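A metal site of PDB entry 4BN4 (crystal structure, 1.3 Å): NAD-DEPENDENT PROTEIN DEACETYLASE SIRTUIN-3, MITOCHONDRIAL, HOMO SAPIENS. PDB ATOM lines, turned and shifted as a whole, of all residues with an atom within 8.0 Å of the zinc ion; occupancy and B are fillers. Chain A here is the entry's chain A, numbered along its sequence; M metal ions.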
ATOM      1  N   THR A 140       9.287  -6.990 -15.660  1.00  0.00           N
ATOM      2  CA  THR A 140       7.859  -6.747 -15.678  1.00  0.00           C
ATOM      3  C   THR A 140       7.134  -8.067 -16.014  1.00  0.00           C
ATOM      4  O   THR A 140       7.483  -8.742 -16.954  1.00  0.00           O
ATOM      5  CB  THR A 140       7.493  -5.584 -16.685  1.00  0.00           C
ATOM      6  OG1 THR A 140       8.220  -4.399 -16.362  1.00  0.00           O
ATOM      7  CG2 THR A 140       5.998  -5.213 -16.599  1.00  0.00           C
ATOM      8  N   CYS A 141       6.087  -8.398 -15.200  1.00  0.00           N
ATOM      9  CA  CYS A 141       5.239  -9.528 -15.544  1.00  0.00           C
ATOM     10  C   CYS A 141       4.544  -9.287 -16.844  1.00  0.00           C
ATOM     11  O   CYS A 141       4.001  -8.220 -17.056  1.00  0.00           O
ATOM     12  CB  CYS A 141       4.237  -9.788 -14.432  1.00  0.00           C
ATOM     13  SG  CYS A 141       3.159 -11.165 -14.871  1.00  0.00           S
ATOM     14  N   THR A 142       4.651 -10.251 -17.752  1.00  0.00           N
ATOM     15  CA  THR A 142       4.028 -10.088 -19.091  1.00  0.00           C
ATOM     16  C   THR A 142       2.519 -10.178 -19.067  1.00  0.00           C
ATOM     17  O   THR A 142       1.889  -9.769 -20.031  1.00  0.00           O
ATOM     18  CB  THR A 142       4.560 -11.129 -20.030  1.00  0.00           C
ATOM     19  OG1 THR A 142       4.350 -12.444 -19.478  1.00  0.00           O
ATOM     20  CG2 THR A 142       6.064 -10.814 -20.307  1.00  0.00           C
ATOM     21  N   VAL A 143       1.943 -10.668 -17.972  1.00  0.00           N
ATOM     22  CA  VAL A 143       0.465 -10.826 -17.854  1.00  0.00           C
ATOM     23  C   VAL A 143      -0.159  -9.686 -17.065  1.00  0.00           C
ATOM     24  O   VAL A 143      -0.950  -8.932 -17.622  1.00  0.00           O
ATOM     25  CB  VAL A 143       0.114 -12.150 -17.203  1.00  0.00           C
ATOM     26  CG1 VAL A 143      -1.412 -12.321 -17.109  1.00  0.00           C
ATOM     27  CG2 VAL A 143       0.714 -13.267 -18.031  1.00  0.00           C
ATOM     28  N   CYS A 144       0.233  -9.531 -15.803  1.00  0.00           N
ATOM     29  CA  CYS A 144      -0.329  -8.511 -14.912  1.00  0.00           C
ATOM     30  C   CYS A 144       0.412  -7.157 -14.910  1.00  0.00           C
ATOM     31  O   CYS A 144      -0.085  -6.154 -14.360  1.00  0.00           O
ATOM     32  CB  CYS A 144      -0.425  -9.117 -13.500  1.00  0.00           C
ATOM     33  SG  CYS A 144       1.116  -9.409 -12.641  1.00  0.00           S
ATOM     34  N   GLN A 145       1.579  -7.125 -15.550  1.00  0.00           N
ATOM     35  CA  GLN A 145       2.356  -5.875 -15.656  1.00  0.00           C
ATOM     36  C   GLN A 145       2.976  -5.401 -14.331  1.00  0.00           C
ATOM     37  O   GLN A 145       3.375  -4.235 -14.218  1.00  0.00           O
ATOM     38  CB  GLN A 145       1.583  -4.738 -16.354  1.00  0.00           C
ATOM     39  CG  GLN A 145       0.998  -5.159 -17.716  1.00  0.00           C
ATOM     40  CD  GLN A 145       2.057  -5.639 -18.703  1.00  0.00           C
ATOM     41  OE1 GLN A 145       3.064  -4.955 -18.950  1.00  0.00           O
ATOM     42  NE2 GLN A 145       1.826  -6.814 -19.295  1.00  0.00           N
ATOM     43  N   ARG A 146       3.025  -6.284 -13.330  1.00  0.00           N
ATOM     44  CA  ARG A 146       3.674  -5.957 -12.049  1.00  0.00           C
ATOM     45  C   ARG A 146       5.161  -5.703 -12.299  1.00  0.00           C
ATOM     46  O   ARG A 146       5.773  -6.478 -13.013  1.00  0.00           O
ATOM     47  CB  ARG A 146       3.488  -7.105 -11.037  1.00  0.00           C
ATOM     48  CG  ARG A 146       4.188  -6.889  -9.709  1.00  0.00           C
ATOM     49  N   PRO A 147       5.727  -4.634 -11.745  1.00  0.00           N
ATOM     50  CA  PRO A 147       7.163  -4.456 -11.900  1.00  0.00           C
ATOM     51  C   PRO A 147       7.897  -5.178 -10.768  1.00  0.00           C
ATOM     52  O   PRO A 147       7.411  -5.321  -9.659  1.00  0.00           O
ATOM     53  CB  PRO A 147       7.334  -2.961 -11.815  1.00  0.00           C
ATOM     54  CG  PRO A 147       6.221  -2.511 -10.895  1.00  0.00           C
ATOM     55  CD  PRO A 147       5.086  -3.439 -11.158  1.00  0.00           C
ATOM     56  N   PHE A 148       9.113  -5.640 -11.101  1.00  0.00           N
ATOM     57  CA  PHE A 148      10.057  -6.298 -10.193  1.00  0.00           C
ATOM     58  C   PHE A 148      11.457  -5.735 -10.370  1.00  0.00           C
ATOM     59  O   PHE A 148      11.896  -5.440 -11.495  1.00  0.00           O
ATOM     60  CB  PHE A 148      10.092  -7.800 -10.406  1.00  0.00           C
ATOM     61  CG  PHE A 148       8.761  -8.454 -10.197  1.00  0.00           C
ATOM     62  CD1 PHE A 148       8.290  -8.747  -8.911  1.00  0.00           C
ATOM     63  CD2 PHE A 148       7.963  -8.758 -11.262  1.00  0.00           C
ATOM     64  CE1 PHE A 148       7.014  -9.347  -8.713  1.00  0.00           C
ATOM     65  CE2 PHE A 148       6.709  -9.350 -11.072  1.00  0.00           C
ATOM     66  CZ  PHE A 148       6.200  -9.635  -9.804  1.00  0.00           C
ATOM     67  N   ARG A 164       8.663 -17.029 -13.055  1.00  0.00           N
ATOM     68  CA  ARG A 164       7.225 -16.815 -13.045  1.00  0.00           C
ATOM     69  C   ARG A 164       6.808 -15.854 -11.943  1.00  0.00           C
ATOM     70  O   ARG A 164       7.418 -15.784 -10.870  1.00  0.00           O
ATOM     71  CB  ARG A 164       6.485 -18.159 -13.011  1.00  0.00           C
ATOM     72  CG  ARG A 164       6.859 -19.039 -14.190  1.00  0.00           C
ATOM     73  CD  ARG A 164       5.624 -19.590 -14.875  1.00  0.00           C
ATOM     74  NE  ARG A 164       5.949 -20.139 -16.176  1.00  0.00           N
ATOM     75  CZ  ARG A 164       5.209 -20.023 -17.279  1.00  0.00           C
ATOM     76  NH1 ARG A 164       4.061 -19.355 -17.263  1.00  0.00           N
ATOM     77  NH2 ARG A 164       5.644 -20.576 -18.406  1.00  0.00           N
ATOM     78  N   CYS A 165       5.792 -15.055 -12.262  1.00  0.00           N
ATOM     79  CA  CYS A 165       5.277 -14.046 -11.376  1.00  0.00           C
ATOM     80  C   CYS A 165       4.651 -14.689 -10.120  1.00  0.00           C
ATOM     81  O   CYS A 165       3.899 -15.650 -10.231  1.00  0.00           O
ATOM     82  CB  CYS A 165       4.197 -13.307 -12.104  1.00  0.00           C
ATOM     83  SG  CYS A 165       3.314 -12.012 -11.197  1.00  0.00           S
ATOM     84  N   PRO A 166       4.944 -14.136  -8.908  1.00  0.00           N
ATOM     85  CA  PRO A 166       4.422 -14.683  -7.643  1.00  0.00           C
ATOM     86  C   PRO A 166       2.900 -14.643  -7.548  1.00  0.00           C
ATOM     87  O   PRO A 166       2.314 -15.497  -6.895  1.00  0.00           O
ATOM     88  CB  PRO A 166       5.055 -13.806  -6.543  1.00  0.00           C
ATOM     89  CG  PRO A 166       5.875 -12.779  -7.232  1.00  0.00           C
ATOM     90  CD  PRO A 166       5.948 -13.075  -8.696  1.00  0.00           C
ATOM     91  N   VAL A 167       2.289 -13.663  -8.204  1.00  0.00           N
ATOM     92  CA  VAL A 167       0.849 -13.515  -8.133  1.00  0.00           C
ATOM     93  C   VAL A 167       0.150 -14.302  -9.237  1.00  0.00           C
ATOM     94  O   VAL A 167      -0.786 -15.037  -8.943  1.00  0.00           O
ATOM     95  CB  VAL A 167       0.411 -12.032  -8.137  1.00  0.00           C
ATOM     96  CG1 VAL A 167       1.436 -11.188  -7.411  1.00  0.00           C
ATOM     97  CG2 VAL A 167       0.170 -11.484  -9.547  1.00  0.00           C
ATOM     98  N   CYS A 168       0.570 -14.171 -10.504  1.00  0.00           N
ATOM     99  CA  CYS A 168      -0.344 -14.628 -11.557  1.00  0.00           C
ATOM    100  C   CYS A 168       0.191 -15.869 -12.335  1.00  0.00           C
ATOM    101  O   CYS A 168      -0.564 -16.536 -13.087  1.00  0.00           O
ATOM    102  CB  CYS A 168      -0.721 -13.447 -12.463  1.00  0.00           C
ATOM    103  SG  CYS A 168       0.490 -12.984 -13.714  1.00  0.00           S
ATOM    104  N   THR A 169       1.456 -16.191 -12.048  1.00  0.00           N
ATOM    105  CA  THR A 169       2.262 -17.284 -12.639  1.00  0.00           C
ATOM    106  C   THR A 169       2.759 -16.934 -14.059  1.00  0.00           C
ATOM    107  O   THR A 169       3.435 -17.759 -14.675  1.00  0.00           O
ATOM    108  CB  THR A 169       1.574 -18.673 -12.619  1.00  0.00           C
ATOM    109  OG1 THR A 169       0.430 -18.654 -13.487  1.00  0.00           O
ATOM    110  CG2 THR A 169       1.181 -19.068 -11.168  1.00  0.00           C
ATOM    111  N   GLY A 170       2.383 -15.752 -14.567  1.00  0.00           N
ATOM    112  CA  GLY A 170       2.881 -15.200 -15.843  1.00  0.00           C
ATOM    113  C   GLY A 170       4.398 -15.145 -15.955  1.00  0.00           C
ATOM    114  O   GLY A 170       5.097 -15.049 -14.960  1.00  0.00           O
ATOM    115  N   VAL A 171       4.909 -15.239 -17.176  1.00  0.00           N
ATOM    116  CA  VAL A 171       6.381 -15.049 -17.370  1.00  0.00           C
ATOM    117  C   VAL A 171       6.775 -13.610 -17.053  1.00  0.00           C
ATOM    118  O   VAL A 171       6.118 -12.669 -17.451  1.00  0.00           O
ATOM    119  CB  VAL A 171       6.827 -15.455 -18.784  1.00  0.00           C
ATOM    120  CG1 VAL A 171       8.295 -15.068 -19.019  1.00  0.00           C
ATOM    121  CG2 VAL A 171       6.635 -16.954 -18.968  1.00  0.00           C
ATOM    122  N   VAL A 172       7.833 -13.511 -16.236  1.00  0.00           N
ATOM    123  CA  VAL A 172       8.394 -12.231 -15.835  1.00  0.00           C
ATOM    124  C   VAL A 172       9.568 -11.968 -16.786  1.00  0.00           C
ATOM    125  O   VAL A 172      10.529 -12.722 -16.865  1.00  0.00           O
ATOM    126  CB  VAL A 172       8.870 -12.181 -14.337  1.00  0.00           C
ATOM    127  CG1 VAL A 172       9.534 -10.830 -14.043  1.00  0.00           C
ATOM    128  CG2 VAL A 172       7.695 -12.431 -13.378  1.00  0.00           C
HETATM  129 ZN    ZN M   1       1.917 -11.451 -12.912  1.00  0.00          ZN
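SG of Cys 144 binds the zinc ion, at 2.2 Å. The side-chain sulfur (SG) of Cys 168 binds the zinc ion, at 2.2 Å. The side-chain sulfur (SG) of Cys 165 is bound to the zinc ion, at 2.3 Å. The side-chain sulfur (SG) of Cys 141 binds the zinc ion.
Merely in contact with the zinc ion: Val 167 (3.8 Å). Within 4 Å of the zinc ion: Cys 141, Cys 144, Cys 165, Val 167 and Cys 168.
SG of Cys 165 sits close to N of Val 167 (3.6 Å). The backbone NH (N) of Cys 141 is in hydrogen-bond range of the backbone carbonyl oxygen (O) of Arg 146. O of Cys 141 lies close to NE2 of Gln 145 (3.4 Å). The side-chain sulfur (SG) of Cys 168 lies close to the backbone NH (N) of Gly 170, 3.5 Å away. O of Gly 170 lies within hydrogen-bond range of N of Cys 165 (2.8 Å). The side-chain sulfur (SG) of Cys 144 sits close to the backbone NH (N) of Arg 146 (3.7 Å). The side-chain sulfur (SG) of Cys 141 sits close to the backbone NH (N) of Val 143 (3.4 Å).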
